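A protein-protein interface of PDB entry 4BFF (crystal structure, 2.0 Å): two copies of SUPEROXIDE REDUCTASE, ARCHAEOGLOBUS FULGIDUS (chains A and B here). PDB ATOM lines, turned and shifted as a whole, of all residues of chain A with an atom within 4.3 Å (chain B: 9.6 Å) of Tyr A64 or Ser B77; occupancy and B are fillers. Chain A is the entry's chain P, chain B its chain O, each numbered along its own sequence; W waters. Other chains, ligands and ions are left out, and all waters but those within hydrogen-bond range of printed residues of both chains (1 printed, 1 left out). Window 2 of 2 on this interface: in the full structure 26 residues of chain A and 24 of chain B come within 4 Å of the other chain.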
ATOM      1  N   VAL A  54      20.200 -25.950 -16.818  1.00  0.00           N
ATOM      2  CA  VAL A  54      20.254 -25.763 -18.261  1.00  0.00           C
ATOM      3  C   VAL A  54      20.082 -27.103 -18.990  1.00  0.00           C
ATOM      4  O   VAL A  54      20.745 -28.073 -18.663  1.00  0.00           O
ATOM      5  CB  VAL A  54      21.607 -25.143 -18.676  1.00  0.00           C
ATOM      6  CG1 VAL A  54      21.830 -25.259 -20.164  1.00  0.00           C
ATOM      7  CG2 VAL A  54      21.678 -23.688 -18.228  1.00  0.00           C
ATOM      8  N   PHE A  55      19.211 -27.159 -19.985  1.00  0.00           N
ATOM      9  CA  PHE A  55      19.061 -28.413 -20.730  1.00  0.00           C
ATOM     10  C   PHE A  55      19.264 -28.181 -22.219  1.00  0.00           C
ATOM     11  O   PHE A  55      18.647 -27.285 -22.806  1.00  0.00           O
ATOM     12  CB  PHE A  55      17.690 -29.045 -20.449  1.00  0.00           C
ATOM     13  CG  PHE A  55      17.373 -30.244 -21.311  1.00  0.00           C
ATOM     14  CD1 PHE A  55      18.137 -31.400 -21.231  1.00  0.00           C
ATOM     15  CD2 PHE A  55      16.286 -30.219 -22.182  1.00  0.00           C
ATOM     16  CE1 PHE A  55      17.838 -32.503 -22.018  1.00  0.00           C
ATOM     17  CE2 PHE A  55      15.975 -31.321 -22.970  1.00  0.00           C
ATOM     18  CZ  PHE A  55      16.753 -32.463 -22.890  1.00  0.00           C
ATOM     19  N   PRO A  57      18.824 -30.327 -25.616  1.00  0.00           N
ATOM     20  CA  PRO A  57      18.375 -31.544 -26.314  1.00  0.00           C
ATOM     21  C   PRO A  57      19.308 -31.943 -27.460  1.00  0.00           C
ATOM     22  O   PRO A  57      19.876 -31.084 -28.140  1.00  0.00           O
ATOM     23  CB  PRO A  57      17.004 -31.154 -26.885  1.00  0.00           C
ATOM     24  CG  PRO A  57      16.590 -29.910 -26.158  1.00  0.00           C
ATOM     25  CD  PRO A  57      17.862 -29.218 -25.737  1.00  0.00           C
ATOM     26  N   SER A  60      19.846 -30.009 -30.871  1.00  0.00           N
ATOM     27  CA  SER A  60      19.669 -28.573 -30.695  1.00  0.00           C
ATOM     28  C   SER A  60      21.010 -27.844 -30.728  1.00  0.00           C
ATOM     29  O   SER A  60      21.908 -28.155 -29.954  1.00  0.00           O
ATOM     30  CB  SER A  60      18.949 -28.269 -29.378  1.00  0.00           C
ATOM     31  OG  SER A  60      18.757 -26.875 -29.208  1.00  0.00           O
ATOM     32  N   PHE A  62      21.565 -24.811 -29.777  1.00  0.00           N
ATOM     33  CA  PHE A  62      21.732 -24.043 -28.541  1.00  0.00           C
ATOM     34  C   PHE A  62      21.084 -24.680 -27.313  1.00  0.00           C
ATOM     35  O   PHE A  62      20.088 -25.387 -27.428  1.00  0.00           O
ATOM     36  CB  PHE A  62      21.202 -22.626 -28.730  1.00  0.00           C
ATOM     37  CG  PHE A  62      21.855 -21.889 -29.866  1.00  0.00           C
ATOM     38  CD1 PHE A  62      23.050 -21.204 -29.673  1.00  0.00           C
ATOM     39  CD2 PHE A  62      21.279 -21.893 -31.125  1.00  0.00           C
ATOM     40  CE1 PHE A  62      23.654 -20.521 -30.713  1.00  0.00           C
ATOM     41  CE2 PHE A  62      21.873 -21.212 -32.182  1.00  0.00           C
ATOM     42  CZ  PHE A  62      23.068 -20.531 -31.978  1.00  0.00           C
ATOM     43  N   PRO A  63      21.658 -24.421 -26.127  1.00  0.00           N
ATOM     44  CA  PRO A  63      21.086 -24.895 -24.867  1.00  0.00           C
ATOM     45  C   PRO A  63      19.959 -23.971 -24.424  1.00  0.00           C
ATOM     46  O   PRO A  63      19.855 -22.845 -24.929  1.00  0.00           O
ATOM     47  CB  PRO A  63      22.258 -24.771 -23.899  1.00  0.00           C
ATOM     48  CG  PRO A  63      23.016 -23.607 -24.406  1.00  0.00           C
ATOM     49  CD  PRO A  63      22.912 -23.673 -25.911  1.00  0.00           C
ATOM     50  N   TYR A  64      19.127 -24.447 -23.501  1.00  0.00           N
ATOM     51  CA  TYR A  64      18.051 -23.633 -22.943  1.00  0.00           C
ATOM     52  C   TYR A  64      18.113 -23.658 -21.420  1.00  0.00           C
ATOM     53  O   TYR A  64      18.346 -24.710 -20.819  1.00  0.00           O
ATOM     54  CB  TYR A  64      16.671 -24.143 -23.392  1.00  0.00           C
ATOM     55  CG  TYR A  64      16.514 -24.222 -24.878  1.00  0.00           C
ATOM     56  CD1 TYR A  64      16.410 -23.064 -25.652  1.00  0.00           C
ATOM     57  CD2 TYR A  64      16.486 -25.446 -25.521  1.00  0.00           C
ATOM     58  CE1 TYR A  64      16.282 -23.136 -27.018  1.00  0.00           C
ATOM     59  CE2 TYR A  64      16.356 -25.524 -26.881  1.00  0.00           C
ATOM     60  CZ  TYR A  64      16.252 -24.376 -27.627  1.00  0.00           C
ATOM     61  OH  TYR A  64      16.131 -24.485 -28.994  1.00  0.00           O
ATOM     62  N   VAL A  65      17.919 -22.506 -20.784  1.00  0.00           N
ATOM     63  CA  VAL A  65      17.764 -22.477 -19.334  1.00  0.00           C
ATOM     64  C   VAL A  65      16.396 -23.048 -18.997  1.00  0.00           C
ATOM     65  O   VAL A  65      15.384 -22.649 -19.590  1.00  0.00           O
ATOM     66  CB  VAL A  65      17.857 -21.048 -18.770  1.00  0.00           C
ATOM     67  CG1 VAL A  65      17.636 -21.058 -17.244  1.00  0.00           C
ATOM     68  CG2 VAL A  65      19.210 -20.422 -19.116  1.00  0.00           C
ATOM     69  N   VAL A  66      16.347 -23.980 -18.067  1.00  0.00           N
ATOM     70  CA  VAL A  66      15.074 -24.571 -17.699  1.00  0.00           C
ATOM     71  C   VAL A  66      14.447 -23.721 -16.611  1.00  0.00           C
ATOM     72  O   VAL A  66      13.283 -23.342 -16.686  1.00  0.00           O
ATOM     73  CB  VAL A  66      15.259 -26.026 -17.227  1.00  0.00           C
ATOM     74  CG1 VAL A  66      13.989 -26.550 -16.633  1.00  0.00           C
ATOM     75  CG2 VAL A  66      15.705 -26.893 -18.392  1.00  0.00           C
ATOM     76  N   THR B  44       4.965 -20.063 -26.019  1.00  0.00           N
ATOM     77  CA  THR B  44       5.943 -18.977 -26.109  1.00  0.00           C
ATOM     78  C   THR B  44       5.267 -17.622 -25.893  1.00  0.00           C
ATOM     79  O   THR B  44       5.900 -16.666 -25.443  1.00  0.00           O
ATOM     80  CB  THR B  44       6.649 -18.980 -27.480  1.00  0.00           C
ATOM     81  OG1 THR B  44       7.155 -20.295 -27.763  1.00  0.00           O
ATOM     82  CG2 THR B  44       7.785 -17.978 -27.496  1.00  0.00           C
ATOM     83  N   PHE B  71      10.582 -20.138 -14.126  1.00  0.00           N
ATOM     84  CA  PHE B  71      10.304 -21.139 -15.175  1.00  0.00           C
ATOM     85  C   PHE B  71      10.586 -20.528 -16.540  1.00  0.00           C
ATOM     86  O   PHE B  71       9.814 -19.711 -17.026  1.00  0.00           O
ATOM     87  CB  PHE B  71       8.854 -21.612 -15.056  1.00  0.00           C
ATOM     88  CG  PHE B  71       8.439 -21.825 -13.636  1.00  0.00           C
ATOM     89  CD1 PHE B  71       9.045 -22.821 -12.879  1.00  0.00           C
ATOM     90  CD2 PHE B  71       7.506 -20.991 -13.035  1.00  0.00           C
ATOM     91  CE1 PHE B  71       8.701 -23.008 -11.558  1.00  0.00           C
ATOM     92  CE2 PHE B  71       7.154 -21.171 -11.712  1.00  0.00           C
ATOM     93  CZ  PHE B  71       7.747 -22.184 -10.975  1.00  0.00           C
ATOM     94  N   ALA B  72      11.704 -20.916 -17.138  1.00  0.00           N
ATOM     95  CA  ALA B  72      12.289 -20.146 -18.233  1.00  0.00           C
ATOM     96  C   ALA B  72      12.072 -20.704 -19.650  1.00  0.00           C
ATOM     97  O   ALA B  72      12.169 -19.961 -20.640  1.00  0.00           O
ATOM     98  CB  ALA B  72      13.795 -19.917 -17.966  1.00  0.00           C
ATOM     99  N   ALA B  73      11.795 -22.000 -19.771  1.00  0.00           N
ATOM    100  CA  ALA B  73      11.626 -22.577 -21.116  1.00  0.00           C
ATOM    101  C   ALA B  73      10.155 -22.660 -21.520  1.00  0.00           C
ATOM    102  O   ALA B  73       9.328 -23.211 -20.784  1.00  0.00           O
ATOM    103  CB  ALA B  73      12.296 -23.937 -21.208  1.00  0.00           C
ATOM    104  N   HIS B  74       9.832 -22.095 -22.683  1.00  0.00           N
ATOM    105  CA  HIS B  74       8.461 -22.022 -23.148  1.00  0.00           C
ATOM    106  C   HIS B  74       8.321 -22.377 -24.650  1.00  0.00           C
ATOM    107  O   HIS B  74       7.508 -21.800 -25.356  1.00  0.00           O
ATOM    108  CB  HIS B  74       7.869 -20.645 -22.832  1.00  0.00           C
ATOM    109  CG  HIS B  74       8.058 -20.222 -21.405  1.00  0.00           C
ATOM    110  ND1 HIS B  74       7.375 -20.799 -20.351  1.00  0.00           N
ATOM    111  CD2 HIS B  74       8.880 -19.293 -20.855  1.00  0.00           C
ATOM    112  CE1 HIS B  74       7.758 -20.233 -19.218  1.00  0.00           C
ATOM    113  NE2 HIS B  74       8.672 -19.319 -19.495  1.00  0.00           N
ATOM    114  N   GLY B  75       9.134 -23.311 -25.128  1.00  0.00           N
ATOM    115  CA  GLY B  75       9.010 -23.832 -26.492  1.00  0.00           C
ATOM    116  C   GLY B  75       9.786 -23.056 -27.550  1.00  0.00           C
ATOM    117  O   GLY B  75       9.877 -23.483 -28.711  1.00  0.00           O
ATOM    118  N   ALA B  76      10.359 -21.915 -27.159  1.00  0.00           N
ATOM    119  CA  ALA B  76      11.001 -21.029 -28.134  1.00  0.00           C
ATOM    120  C   ALA B  76      12.275 -21.650 -28.697  1.00  0.00           C
ATOM    121  O   ALA B  76      13.113 -22.168 -27.941  1.00  0.00           O
ATOM    122  CB  ALA B  76      11.306 -19.665 -27.505  1.00  0.00           C
ATOM    123  N   SER B  77      12.425 -21.590 -30.021  1.00  0.00           N
ATOM    124  CA  SER B  77      13.670 -22.006 -30.669  1.00  0.00           C
ATOM    125  C   SER B  77      13.956 -21.240 -31.963  1.00  0.00           C
ATOM    126  O   SER B  77      13.109 -20.498 -32.462  1.00  0.00           O
ATOM    127  CB  SER B  77      13.648 -23.501 -30.989  1.00  0.00           C
ATOM    128  OG  SER B  77      13.209 -23.722 -32.316  1.00  0.00           O
ATOM    129  N   VAL B  78      15.148 -21.456 -32.514  1.00  0.00           N
ATOM    130  CA  VAL B  78      15.484 -20.917 -33.830  1.00  0.00           C
ATOM    131  C   VAL B  78      14.489 -21.336 -34.935  1.00  0.00           C
ATOM    132  O   VAL B  78      14.308 -20.608 -35.917  1.00  0.00           O
ATOM    133  CB  VAL B  78      16.939 -21.259 -34.247  1.00  0.00           C
ATOM    134  CG1 VAL B  78      17.937 -20.665 -33.235  1.00  0.00           C
ATOM    135  CG2 VAL B  78      17.135 -22.770 -34.381  1.00  0.00           C
ATOM    136  N   ASP B  79      13.826 -22.480 -34.775  1.00  0.00           N
ATOM    137  CA  ASP B  79      12.838 -22.900 -35.778  1.00  0.00           C
ATOM    138  C   ASP B  79      11.494 -22.175 -35.648  1.00  0.00           C
ATOM    139  O   ASP B  79      10.642 -22.293 -36.529  1.00  0.00           O
ATOM    140  CB  ASP B  79      12.608 -24.419 -35.758  1.00  0.00           C
ATOM    141  CG  ASP B  79      13.832 -25.207 -36.182  1.00  0.00           C
ATOM    142  OD1 ASP B  79      14.552 -24.759 -37.100  1.00  0.00           O
ATOM    143  OD2 ASP B  79      14.073 -26.279 -35.592  1.00  0.00           O
ATOM    144  N   GLY B  80      11.303 -21.438 -34.554  1.00  0.00           N
ATOM    145  CA  GLY B  80      10.096 -20.648 -34.367  1.00  0.00           C
ATOM    146  C   GLY B  80       9.492 -20.921 -33.003  1.00  0.00           C
ATOM    147  O   GLY B  80      10.019 -21.742 -32.266  1.00  0.00           O
ATOM    148  N   PRO B  81       8.396 -20.226 -32.655  1.00  0.00           N
ATOM    149  CA  PRO B  81       7.712 -20.439 -31.366  1.00  0.00           C
ATOM    150  C   PRO B  81       7.097 -21.831 -31.219  1.00  0.00           C
ATOM    151  O   PRO B  81       6.607 -22.393 -32.193  1.00  0.00           O
ATOM    152  CB  PRO B  81       6.602 -19.373 -31.361  1.00  0.00           C
ATOM    153  CG  PRO B  81       6.455 -18.955 -32.785  1.00  0.00           C
ATOM    154  CD  PRO B  81       7.809 -19.110 -33.408  1.00  0.00           C
ATOM    155  N   ASN B  82       7.140 -22.365 -30.003  1.00  0.00           N
ATOM    156  CA  ASN B  82       6.591 -23.674 -29.687  1.00  0.00           C
ATOM    157  C   ASN B  82       7.145 -24.822 -30.528  1.00  0.00           C
ATOM    158  O   ASN B  82       6.393 -25.719 -30.936  1.00  0.00           O
ATOM    159  CB  ASN B  82       5.070 -23.642 -29.798  1.00  0.00           C
ATOM    160  CG  ASN B  82       4.467 -22.473 -29.060  1.00  0.00           C
ATOM    161  OD1 ASN B  82       4.495 -22.433 -27.838  1.00  0.00           O
ATOM    162  ND2 ASN B  82       3.901 -21.519 -29.801  1.00  0.00           N
ATOM    163  N   THR B  83       8.452 -24.799 -30.770  1.00  0.00           N
ATOM    164  CA  THR B  83       9.109 -25.825 -31.581  1.00  0.00           C
ATOM    165  C   THR B  83      10.234 -26.564 -30.861  1.00  0.00           C
ATOM    166  O   THR B  83      10.755 -27.538 -31.391  1.00  0.00           O
ATOM    167  CB  THR B  83       9.753 -25.225 -32.850  1.00  0.00           C
ATOM    168  OG1 THR B  83      10.638 -24.159 -32.476  1.00  0.00           O
ATOM    169  CG2 THR B  83       8.689 -24.703 -33.833  1.00  0.00           C
ATOM    170  N   SER B  84      10.628 -26.104 -29.673  1.00  0.00           N
ATOM    171  CA  SER B  84      11.814 -26.666 -29.027  1.00  0.00           C
ATOM    172  C   SER B  84      11.522 -27.953 -28.256  1.00  0.00           C
ATOM    173  O   SER B  84      12.436 -28.730 -27.961  1.00  0.00           O
ATOM    174  CB  SER B  84      12.489 -25.631 -28.093  1.00  0.00           C
ATOM    175  OG  SER B  84      11.921 -25.663 -26.795  1.00  0.00           O
ATOM    176  N   GLY B  85      10.253 -28.170 -27.922  1.00  0.00           N
ATOM    177  CA  GLY B  85       9.857 -29.338 -27.150  1.00  0.00           C
ATOM    178  C   GLY B  85      10.172 -29.253 -25.661  1.00  0.00           C
ATOM    179  O   GLY B  85       9.866 -30.182 -24.894  1.00  0.00           O
ATOM    180  N   VAL B  86      10.779 -28.147 -25.243  1.00  0.00           N
ATOM    181  CA  VAL B  86      11.122 -27.956 -23.821  1.00  0.00           C
ATOM    182  C   VAL B  86      10.206 -26.922 -23.156  1.00  0.00           C
ATOM    183  O   VAL B  86      10.197 -25.744 -23.542  1.00  0.00           O
ATOM    184  CB  VAL B  86      12.609 -27.556 -23.635  1.00  0.00           C
ATOM    185  CG1 VAL B  86      12.958 -27.402 -22.136  1.00  0.00           C
ATOM    186  CG2 VAL B  86      13.540 -28.569 -24.298  1.00  0.00           C
ATOM    187  N   TYR B  87       9.427 -27.359 -22.163  1.00  0.00           N
ATOM    188  CA  TYR B  87       8.503 -26.457 -21.471  1.00  0.00           C
ATOM    189  C   TYR B  87       8.592 -26.599 -19.944  1.00  0.00           C
ATOM    190  O   TYR B  87       8.345 -27.678 -19.421  1.00  0.00           O
ATOM    191  CB  TYR B  87       7.068 -26.712 -21.959  1.00  0.00           C
ATOM    192  CG  TYR B  87       6.856 -26.503 -23.450  1.00  0.00           C
ATOM    193  CD1 TYR B  87       7.186 -27.496 -24.372  1.00  0.00           C
ATOM    194  CD2 TYR B  87       6.286 -25.331 -23.931  1.00  0.00           C
ATOM    195  CE1 TYR B  87       6.984 -27.314 -25.733  1.00  0.00           C
ATOM    196  CE2 TYR B  87       6.080 -25.137 -25.287  1.00  0.00           C
ATOM    197  CZ  TYR B  87       6.435 -26.133 -26.183  1.00  0.00           C
ATOM    198  OH  TYR B  87       6.232 -25.948 -27.533  1.00  0.00           O
ATOM    199  N   THR B  88       8.953 -25.530 -19.226  1.00  0.00           N
ATOM    200  CA  THR B  88       9.096 -25.642 -17.765  1.00  0.00           C
ATOM    201  C   THR B  88       7.738 -25.581 -17.034  1.00  0.00           C
ATOM    202  O   THR B  88       7.035 -24.576 -17.120  1.00  0.00           O
ATOM    203  CB  THR B  88      10.041 -24.552 -17.167  1.00  0.00           C
ATOM    204  OG1 THR B  88      11.257 -24.462 -17.939  1.00  0.00           O
ATOM    205  CG2 THR B  88      10.365 -24.867 -15.688  1.00  0.00           C
HETATM  206  O   HOH W   1      17.245 -22.433 -30.474  1.00  0.00           O
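A ring nitrogen (NE2) of His B74 lies within hydrogen-bond range of the backbone carbonyl oxygen (O) of Phe B71 (2.7 Å).
The backbone NH of Ser B84 sits at hydrogen-bond distance from the backbone carbonyl oxygen of Gly B75 (2.9 Å).
The backbone carbonyl oxygen of Val B86 sits at hydrogen-bond distance from the backbone NH of Gly B75 (3.1 Å).
The side-chain hydroxyl (OG) of Ser B77 sits at hydrogen-bond distance from the backbone NH (N) of Asp B79 (2.8 Å).
The side-chain hydroxyl (OG1) of Thr B83 is in hydrogen-bond range of the side-chain hydroxyl (OG) of Ser B77.
The side-chain hydroxyl (OG) of Ser B84 lies close to the backbone NH (N) of Val B86 (3.1 Å).
The backbone NH (N) of Ala B72 lies within hydrogen-bond range of the backbone carbonyl oxygen (O) of Val A66 (2.9 Å).
O of Val A66 sits at hydrogen-bond distance from OG1 of Thr B88 (2.6 Å).
No position is printed for both chains.
Of the 11 pairs that touch across the chains among the printed residues, none has its exchanged pair printed and touching as well.
Of chain B, only Ala B76 (3.4 Å), Ser B77 (3.3 Å) and Ser B84 (3.9 Å) come within 4 Å of Tyr A64.
Ser B77 touches just one residue of chain A: Tyr A64.
No residue of chain B comes within 4 Å of Pro A63.
Of the printed residues of chain B, Val A66 touches Phe B71, Ala B72, Ala B73 and Thr B88.
Of the printed residues of chain B, Val A65 touches Ala B72 and Ala B73.
Of the printed residues of chain A, Ala B76 touches Tyr A64 (3.4 Å).
Ser A60 touches none of the printed residues of chain B.
Phe A62 touches none of the printed residues of chain B.
The nearest printed residue of chain B that does not touch Phe A55 is Gly B85 (6.5 Å).
Water W1 bridges the side-chain hydroxyl of Tyr A64 (2.8 Å) and the backbone NH of Val B78 (3.1 Å).
Among the printed residues, merely in contact across the chains: Phe A55 with Val B86 (3.8 Å), Pro A57 with Val B86 (3.8 Å), Tyr A64 with Ala B76 (3.4 Å), Tyr A64 with Ser B77 (3.3 Å), Tyr A64 with Ser B84 (3.9 Å), Val A65 with Ala B72 (3.6 Å), Val A65 with Ala B73 (3.7 Å), Val A66 with Phe B71 (3.9 Å) and Val A66 with Ala B73 (3.7 Å).
Of the 19 printed residues of chain B, 8 touch a printed residue of chain A.
Printed residues of chain B that touch a printed residue of chain A: Phe B71, Ala B72, Ala B73, Ala B76, Ser B77, Ser B84, Val B86 and Thr B88.
Hydrophobic or aromatic side chains of chain B that line the printed part of chain A: Ala B72, Ala B73 and Val B86.
Among the printed residues, no Asp or Glu carboxylate lies within 4 Å of a Lys or Arg side-chain nitrogen of the other chain.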
